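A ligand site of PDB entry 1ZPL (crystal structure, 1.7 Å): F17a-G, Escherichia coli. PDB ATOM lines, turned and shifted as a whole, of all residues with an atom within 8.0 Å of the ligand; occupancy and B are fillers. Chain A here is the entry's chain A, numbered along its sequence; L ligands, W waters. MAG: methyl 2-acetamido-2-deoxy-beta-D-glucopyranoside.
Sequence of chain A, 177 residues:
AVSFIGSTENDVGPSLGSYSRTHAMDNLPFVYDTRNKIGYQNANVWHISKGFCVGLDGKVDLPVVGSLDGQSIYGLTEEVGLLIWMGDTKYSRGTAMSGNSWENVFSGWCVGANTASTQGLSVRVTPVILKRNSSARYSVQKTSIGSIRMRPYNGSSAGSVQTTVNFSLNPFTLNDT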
ATOM      1  N   ASN A  42       1.608   2.639  19.764  1.00  0.00           N
ATOM      2  CA  ASN A  42       2.178   3.243  20.954  1.00  0.00           C
ATOM      3  C   ASN A  42       1.039   3.498  21.934  1.00  0.00           C
ATOM      4  O   ASN A  42       0.175   4.338  21.690  1.00  0.00           O
ATOM      5  CB  ASN A  42       2.866   4.579  20.607  1.00  0.00           C
ATOM      6  CG  ASN A  42       3.747   5.082  21.732  1.00  0.00           C
ATOM      7  OD1 ASN A  42       3.478   4.842  22.908  1.00  0.00           O
ATOM      8  ND2 ASN A  42       4.803   5.813  21.380  1.00  0.00           N
ATOM      9  N   ALA A  43       1.048   2.766  23.042  1.00  0.00           N
ATOM     10  CA  ALA A  43       0.000   2.903  24.051  1.00  0.00           C
ATOM     11  C   ALA A  43       0.128   4.154  24.905  1.00  0.00           C
ATOM     12  O   ALA A  43      -0.815   4.527  25.612  1.00  0.00           O
ATOM     13  CB  ALA A  43      -0.008   1.660  24.944  1.00  0.00           C
ATOM     14  N   ASN A  44       1.283   4.819  24.833  1.00  0.00           N
ATOM     15  CA  ASN A  44       1.503   6.008  25.664  1.00  0.00           C
ATOM     16  C   ASN A  44       1.940   7.235  24.875  1.00  0.00           C
ATOM     17  O   ASN A  44       3.120   7.556  24.832  1.00  0.00           O
ATOM     18  CB  ASN A  44       2.547   5.685  26.726  1.00  0.00           C
ATOM     19  CG  ASN A  44       2.305   4.338  27.376  1.00  0.00           C
ATOM     20  OD1 ASN A  44       2.963   3.350  27.050  1.00  0.00           O
ATOM     21  ND2 ASN A  44       1.342   4.280  28.293  1.00  0.00           N
ATOM     22  N   VAL A  45       0.986   7.940  24.278  1.00  0.00           N
ATOM     23  CA  VAL A  45       1.292   9.136  23.498  1.00  0.00           C
ATOM     24  C   VAL A  45       0.962  10.403  24.290  1.00  0.00           C
ATOM     25  O   VAL A  45       1.658  11.405  24.162  1.00  0.00           O
ATOM     26  CB  VAL A  45       0.534   9.120  22.157  1.00  0.00           C
ATOM     27  CG1 VAL A  45       0.776  10.419  21.391  1.00  0.00           C
ATOM     28  CG2 VAL A  45       1.016   7.927  21.331  1.00  0.00           C
ATOM     29  N   TRP A  46      -0.093  10.332  25.088  1.00  0.00           N
ATOM     30  CA  TRP A  46      -0.484  11.454  25.939  1.00  0.00           C
ATOM     31  C   TRP A  46      -0.719  10.915  27.337  1.00  0.00           C
ATOM     32  O   TRP A  46      -1.241   9.816  27.500  1.00  0.00           O
ATOM     33  CB  TRP A  46      -1.784  12.104  25.474  1.00  0.00           C
ATOM     34  CG  TRP A  46      -1.684  12.877  24.211  1.00  0.00           C
ATOM     35  CD1 TRP A  46      -1.249  14.164  24.059  1.00  0.00           C
ATOM     36  CD2 TRP A  46      -1.966  12.385  22.898  1.00  0.00           C
ATOM     37  NE1 TRP A  46      -1.249  14.497  22.725  1.00  0.00           N
ATOM     38  CE2 TRP A  46      -1.688  13.434  21.993  1.00  0.00           C
ATOM     39  CE3 TRP A  46      -2.440  11.159  22.400  1.00  0.00           C
ATOM     40  CZ2 TRP A  46      -1.847  13.284  20.616  1.00  0.00           C
ATOM     41  CZ3 TRP A  46      -2.599  11.025  21.030  1.00  0.00           C
ATOM     42  CH2 TRP A  46      -2.310  12.080  20.153  1.00  0.00           C
ATOM     43  N   ILE A  48      -2.774  11.365  30.658  1.00  0.00           N
ATOM     44  CA  ILE A  48      -3.988  12.041  31.091  1.00  0.00           C
ATOM     45  C   ILE A  48      -4.353  11.671  32.516  1.00  0.00           C
ATOM     46  O   ILE A  48      -4.004  10.592  32.998  1.00  0.00           O
ATOM     47  CB  ILE A  48      -5.174  11.685  30.165  1.00  0.00           C
ATOM     48  CG1 ILE A  48      -5.423  10.182  30.181  1.00  0.00           C
ATOM     49  CG2 ILE A  48      -4.868  12.140  28.739  1.00  0.00           C
ATOM     50  CD1 ILE A  48      -6.664   9.762  29.399  1.00  0.00           C
ATOM     51  N   VAL A  54     -10.789  12.107  26.403  1.00  0.00           N
ATOM     52  CA  VAL A  54     -10.111  12.291  25.130  1.00  0.00           C
ATOM     53  C   VAL A  54     -10.372  11.162  24.127  1.00  0.00           C
ATOM     54  O   VAL A  54     -10.464   9.989  24.508  1.00  0.00           O
ATOM     55  CB  VAL A  54      -8.586  12.400  25.349  1.00  0.00           C
ATOM     56  CG1 VAL A  54      -8.062  11.108  25.939  1.00  0.00           C
ATOM     57  CG2 VAL A  54      -7.887  12.717  24.046  1.00  0.00           C
ATOM     58  N   LEU A  56      -9.755  10.377  19.528  1.00  0.00           N
ATOM     59  CA  LEU A  56      -8.758  10.615  18.478  1.00  0.00           C
ATOM     60  C   LEU A  56      -9.376  10.886  17.112  1.00  0.00           C
ATOM     61  O   LEU A  56     -10.397  10.281  16.752  1.00  0.00           O
ATOM     62  CB  LEU A  56      -7.833   9.417  18.334  1.00  0.00           C
ATOM     63  CG  LEU A  56      -7.023   8.885  19.522  1.00  0.00           C
ATOM     64  CD1 LEU A  56      -6.486   7.507  19.168  1.00  0.00           C
ATOM     65  CD2 LEU A  56      -5.882   9.837  19.851  1.00  0.00           C
ATOM     66  N   GLY A  87      -6.514   4.558  14.727  1.00  0.00           N
ATOM     67  CA  GLY A  87      -7.401   4.445  15.872  1.00  0.00           C
ATOM     68  C   GLY A  87      -6.691   4.296  17.203  1.00  0.00           C
ATOM     69  O   GLY A  87      -5.540   4.707  17.352  1.00  0.00           O
ATOM     70  N   ASP A  88      -7.402   3.714  18.167  1.00  0.00           N
ATOM     71  CA  ASP A  88      -6.866   3.504  19.502  1.00  0.00           C
ATOM     72  C   ASP A  88      -5.700   2.523  19.449  1.00  0.00           C
ATOM     73  O   ASP A  88      -5.455   1.863  18.427  1.00  0.00           O
ATOM     74  CB  ASP A  88      -7.971   2.984  20.426  1.00  0.00           C
ATOM     75  CG  ASP A  88      -7.616   3.127  21.904  1.00  0.00           C
ATOM     76  OD1 ASP A  88      -6.857   4.057  22.251  1.00  0.00           O
ATOM     77  OD2 ASP A  88      -8.101   2.318  22.710  1.00  0.00           O
ATOM     78  N   THR A  89      -4.973   2.429  20.557  1.00  0.00           N
ATOM     79  CA  THR A  89      -3.802   1.578  20.680  1.00  0.00           C
ATOM     80  C   THR A  89      -3.861   0.195  20.026  1.00  0.00           C
ATOM     81  O   THR A  89      -3.073  -0.089  19.120  1.00  0.00           O
ATOM     82  CB  THR A  89      -3.448   1.378  22.160  1.00  0.00           C
ATOM     83  OG1 THR A  89      -3.257   2.658  22.777  1.00  0.00           O
ATOM     84  CG2 THR A  89      -2.159   0.571  22.287  1.00  0.00           C
ATOM     85  N   LYS A  90      -4.771  -0.668  20.478  1.00  0.00           N
ATOM     86  CA  LYS A  90      -4.879  -2.013  19.928  1.00  0.00           C
ATOM     87  C   LYS A  90      -5.313  -2.031  18.473  1.00  0.00           C
ATOM     88  O   LYS A  90      -6.330  -1.432  18.101  1.00  0.00           O
ATOM     89  CB  LYS A  90      -5.821  -2.849  20.795  1.00  0.00           C
ATOM     90  CG  LYS A  90      -5.261  -3.084  22.200  1.00  0.00           C
ATOM     91  CD  LYS A  90      -6.205  -3.838  23.111  1.00  0.00           C
ATOM     92  CE  LYS A  90      -5.575  -4.005  24.485  1.00  0.00           C
ATOM     93  NZ  LYS A  90      -6.515  -4.633  25.454  1.00  0.00           N
ATOM     94  N   ARG A  93      -8.817  -2.307  16.878  1.00  0.00           N
ATOM     95  CA  ARG A  93      -9.748  -1.188  17.032  1.00  0.00           C
ATOM     96  C   ARG A  93      -9.529  -0.087  16.018  1.00  0.00           C
ATOM     97  O   ARG A  93     -10.093   1.004  16.138  1.00  0.00           O
ATOM     98  CB  ARG A  93      -9.659  -0.647  18.460  1.00  0.00           C
ATOM     99  CG  ARG A  93     -10.479  -1.515  19.405  1.00  0.00           C
ATOM    100  CD  ARG A  93     -10.089  -1.353  20.826  1.00  0.00           C
ATOM    101  NE  ARG A  93     -10.268  -2.624  21.512  1.00  0.00           N
ATOM    102  CZ  ARG A  93      -9.956  -2.826  22.790  1.00  0.00           C
ATOM    103  NH1 ARG A  93      -9.461  -1.839  23.518  1.00  0.00           N
ATOM    104  NH2 ARG A  93     -10.123  -4.032  23.318  1.00  0.00           N
ATOM    105  N   PHE A 106     -11.555   7.154  17.035  1.00  0.00           N
ATOM    106  CA  PHE A 106     -11.685   6.560  18.367  1.00  0.00           C
ATOM    107  C   PHE A 106     -12.630   7.460  19.155  1.00  0.00           C
ATOM    108  O   PHE A 106     -12.273   8.582  19.512  1.00  0.00           O
ATOM    109  CB  PHE A 106     -10.326   6.460  19.071  1.00  0.00           C
ATOM    110  CG  PHE A 106     -10.417   6.043  20.512  1.00  0.00           C
ATOM    111  CD1 PHE A 106     -11.198   4.953  20.895  1.00  0.00           C
ATOM    112  CD2 PHE A 106      -9.727   6.740  21.503  1.00  0.00           C
ATOM    113  CE1 PHE A 106     -11.305   4.572  22.232  1.00  0.00           C
ATOM    114  CE2 PHE A 106      -9.814   6.359  22.850  1.00  0.00           C
ATOM    115  CZ  PHE A 106     -10.596   5.283  23.216  1.00  0.00           C
ATOM    116  N   GLY A 108     -13.376   7.633  22.063  1.00  0.00           N
ATOM    117  CA  GLY A 108     -12.804   8.163  23.291  1.00  0.00           C
ATOM    118  C   GLY A 108     -13.219   7.559  24.620  1.00  0.00           C
ATOM    119  O   GLY A 108     -14.101   6.703  24.704  1.00  0.00           O
ATOM    120  N   TRP A 109     -12.560   8.030  25.677  1.00  0.00           N
ATOM    121  CA  TRP A 109     -12.839   7.573  27.036  1.00  0.00           C
ATOM    122  C   TRP A 109     -12.378   8.643  28.016  1.00  0.00           C
ATOM    123  O   TRP A 109     -11.687   9.586  27.641  1.00  0.00           O
ATOM    124  CB  TRP A 109     -12.102   6.270  27.343  1.00  0.00           C
ATOM    125  CG  TRP A 109     -10.611   6.436  27.537  1.00  0.00           C
ATOM    126  CD1 TRP A 109      -9.712   6.925  26.626  1.00  0.00           C
ATOM    127  CD2 TRP A 109      -9.863   6.111  28.708  1.00  0.00           C
ATOM    128  NE1 TRP A 109      -8.446   6.908  27.168  1.00  0.00           N
ATOM    129  CE2 TRP A 109      -8.506   6.417  28.447  1.00  0.00           C
ATOM    130  CE3 TRP A 109     -10.199   5.584  29.973  1.00  0.00           C
ATOM    131  CZ2 TRP A 109      -7.483   6.213  29.388  1.00  0.00           C
ATOM    132  CZ3 TRP A 109      -9.187   5.384  30.907  1.00  0.00           C
ATOM    133  CH2 TRP A 109      -7.842   5.699  30.601  1.00  0.00           C
ATOM    134  N   CYS A 110     -12.790   8.490  29.275  1.00  0.00           N
ATOM    135  CA  CYS A 110     -12.400   9.440  30.301  1.00  0.00           C
ATOM    136  C   CYS A 110     -11.668   8.710  31.412  1.00  0.00           C
ATOM    137  O   CYS A 110     -12.128   7.678  31.886  1.00  0.00           O
ATOM    138  CB  CYS A 110     -13.631  10.116  30.903  1.00  0.00           C
ATOM    139  SG  CYS A 110     -14.773  10.961  29.774  1.00  0.00           S
ATOM    140  N   VAL A 111     -10.524   9.257  31.825  1.00  0.00           N
ATOM    141  CA  VAL A 111      -9.739   8.662  32.887  1.00  0.00           C
ATOM    142  C   VAL A 111     -10.407   9.022  34.219  1.00  0.00           C
ATOM    143  O   VAL A 111     -11.165   9.995  34.291  1.00  0.00           O
ATOM    144  CB  VAL A 111      -8.278   9.185  32.855  1.00  0.00           C
ATOM    145  CG1 VAL A 111      -8.232  10.675  33.133  1.00  0.00           C
ATOM    146  CG2 VAL A 111      -7.430   8.415  33.854  1.00  0.00           C
ATOM    147  N   ALA A 116      -4.474   8.383  37.097  1.00  0.00           N
ATOM    148  CA  ALA A 116      -3.697   8.783  35.942  1.00  0.00           C
ATOM    149  C   ALA A 116      -3.512   7.591  35.008  1.00  0.00           C
ATOM    150  O   ALA A 116      -3.395   6.448  35.462  1.00  0.00           O
ATOM    151  CB  ALA A 116      -2.334   9.313  36.377  1.00  0.00           C
ATOM    152  N   SER A 117      -3.493   7.859  33.718  1.00  0.00           N
ATOM    153  CA  SER A 117      -3.321   6.812  32.730  1.00  0.00           C
ATOM    154  C   SER A 117      -2.746   7.450  31.469  1.00  0.00           C
ATOM    155  O   SER A 117      -2.154   8.526  31.532  1.00  0.00           O
ATOM    156  CB  SER A 117      -4.657   6.130  32.419  1.00  0.00           C
ATOM    157  OG  SER A 117      -4.474   5.001  31.583  1.00  0.00           O
ATOM    158  N   THR A 118      -2.916   6.778  30.347  1.00  0.00           N
ATOM    159  CA  THR A 118      -2.404   7.305  29.098  1.00  0.00           C
ATOM    160  C   THR A 118      -3.371   7.055  27.951  1.00  0.00           C
ATOM    161  O   THR A 118      -4.313   6.264  28.065  1.00  0.00           O
ATOM    162  CB  THR A 118      -1.062   6.644  28.720  1.00  0.00           C
ATOM    163  OG1 THR A 118      -1.255   5.244  28.533  1.00  0.00           O
ATOM    164  CG2 THR A 118      -0.021   6.883  29.816  1.00  0.00           C
ATOM    165  N   GLN A 119      -3.140   7.761  26.855  1.00  0.00           N
ATOM    166  CA  GLN A 119      -3.944   7.631  25.644  1.00  0.00           C
ATOM    167  C   GLN A 119      -2.949   7.278  24.554  1.00  0.00           C
ATOM    168  O   GLN A 119      -1.940   7.962  24.394  1.00  0.00           O
ATOM    169  CB  GLN A 119      -4.648   8.941  25.305  1.00  0.00           C
ATOM    170  CG  GLN A 119      -5.373   8.929  23.969  1.00  0.00           C
ATOM    171  CD  GLN A 119      -6.379   7.806  23.854  1.00  0.00           C
ATOM    172  OE1 GLN A 119      -7.244   7.642  24.705  1.00  0.00           O
ATOM    173  NE2 GLN A 119      -6.267   7.004  22.789  1.00  0.00           N
ATOM    174  N   GLY A 120      -3.210   6.192  23.835  1.00  0.00           N
ATOM    175  CA  GLY A 120      -2.306   5.779  22.785  1.00  0.00           C
ATOM    176  C   GLY A 120      -2.967   5.822  21.420  1.00  0.00           C
ATOM    177  O   GLY A 120      -4.029   6.421  21.260  1.00  0.00           O
ATOM    178  N   LEU A 121      -2.342   5.185  20.450  1.00  0.00           N
ATOM    179  CA  LEU A 121      -2.870   5.153  19.101  1.00  0.00           C
ATOM    180  C   LEU A 121      -2.182   4.069  18.274  1.00  0.00           C
ATOM    181  O   LEU A 121      -1.215   3.459  18.729  1.00  0.00           O
ATOM    182  CB  LEU A 121      -2.669   6.523  18.432  1.00  0.00           C
ATOM    183  CG  LEU A 121      -1.250   7.110  18.415  1.00  0.00           C
ATOM    184  CD1 LEU A 121      -0.372   6.362  17.421  1.00  0.00           C
ATOM    185  CD2 LEU A 121      -1.306   8.580  18.046  1.00  0.00           C
ATOM    186  N   SER A 122      -2.684   3.850  17.070  1.00  0.00           N
ATOM    187  CA  SER A 122      -2.085   2.879  16.181  1.00  0.00           C
ATOM    188  C   SER A 122      -2.444   3.230  14.746  1.00  0.00           C
ATOM    189  O   SER A 122      -3.496   3.806  14.467  1.00  0.00           O
ATOM    190  CB  SER A 122      -2.575   1.453  16.490  1.00  0.00           C
ATOM    191  OG  SER A 122      -3.932   1.280  16.147  1.00  0.00           O
HETATM  192  C1  MAG L   1      -5.407   2.979  28.386  1.00  0.00           C
HETATM  193  C2  MAG L   1      -4.194   2.593  27.466  1.00  0.00           C
HETATM  194  C3  MAG L   1      -4.118   3.570  26.315  1.00  0.00           C
HETATM  195  C4  MAG L   1      -5.427   3.554  25.557  1.00  0.00           C
HETATM  196  C5  MAG L   1      -6.598   3.903  26.512  1.00  0.00           C
HETATM  197  C6  MAG L   1      -7.955   3.870  25.779  1.00  0.00           C
HETATM  198  C7  MAG L   1      -2.230   1.541  28.494  1.00  0.00           C
HETATM  199  C8  MAG L   1      -0.965   1.785  29.286  1.00  0.00           C
HETATM  200  N2  MAG L   1      -2.944   2.648  28.227  1.00  0.00           N
HETATM  201  O1  MAG L   1      -5.512   2.064  29.429  1.00  0.00           O
HETATM  202  O3  MAG L   1      -3.063   3.246  25.465  1.00  0.00           O
HETATM  203  O4  MAG L   1      -5.363   4.480  24.475  1.00  0.00           O
HETATM  204  O5  MAG L   1      -6.654   2.980  27.597  1.00  0.00           O
HETATM  205  O6  MAG L   1      -8.240   2.571  25.305  1.00  0.00           O
HETATM  206  O7  MAG L   1      -2.530   0.375  28.148  1.00  0.00           O
HETATM  207  CM  MAG L   1      -6.352   2.380  30.296  1.00  0.00           C
HETATM  208  O   HOH W   1      -3.021  -0.253  25.317  1.00  0.00           O
HETATM  209  O   HOH W   2      -0.028  -1.481  28.330  1.00  0.00           O
HETATM  210  O   HOH W   3       1.194   3.508  30.840  1.00  0.00           O
HETATM  211  O   HOH W   4      -3.741  -0.091  31.153  1.00  0.00           O
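O of Ile 48 is in hydrogen-bond range of N of Ser 117 (2.9 Å). The side-chain amide oxygen of Gln 119 is in hydrogen-bond range of the indole nitrogen of Trp 109 (2.8 Å). The backbone carbonyl oxygen (O) of Gln 119 is in hydrogen-bond range of the backbone NH (N) of Val 45 (2.9 Å). The side-chain amide nitrogen (ND2) of Asn 44 is in hydrogen-bond range of the side-chain hydroxyl (OG1) of Thr 118 (2.8 Å). The backbone NH of Val 54 lies within hydrogen-bond range of the backbone carbonyl oxygen of Trp 109. OG1 of Thr 118 lies within hydrogen-bond range of O of Ala 43, 3.0 Å away. The side-chain carboxylate (OD1) of Asp 88 sits at hydrogen-bond distance from the side-chain amide nitrogen (NE2) of Gln 119 (3.1 Å). The side-chain hydroxyl (OG) of Ser 122 sits close to the backbone carbonyl oxygen (O) of Thr 89, 3.4 Å away.
Residues that only touch the ligand: Asn 44 (3.5 Å), Phe 106 (3.9 Å), Trp 109 (3.4 Å) and Ser 117 (3.5 Å). Hydrophobic or aromatic side chains that line the ligand: Ala 43, Phe 106 and Trp 109.
An oxygen (O3) of the ligand sits at hydrogen-bond distance from the side-chain hydroxyl of Thr 89 (2.8 Å). OD2 of Asp 88 is in hydrogen-bond range of O6 of the ligand, 2.6 Å away. The side-chain amide nitrogen of Gln 119 is in hydrogen-bond range of an oxygen (O4) of the ligand (3.2 Å). O4 of the ligand sits at hydrogen-bond distance from N of Gly 120 (2.8 Å). The backbone carbonyl oxygen (O) of Ala 43 sits at hydrogen-bond distance from an oxygen (O3) of the ligand, 2.6 Å away. OG1 of Thr 118 lies within hydrogen-bond range of N2 of the ligand (3.1 Å).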
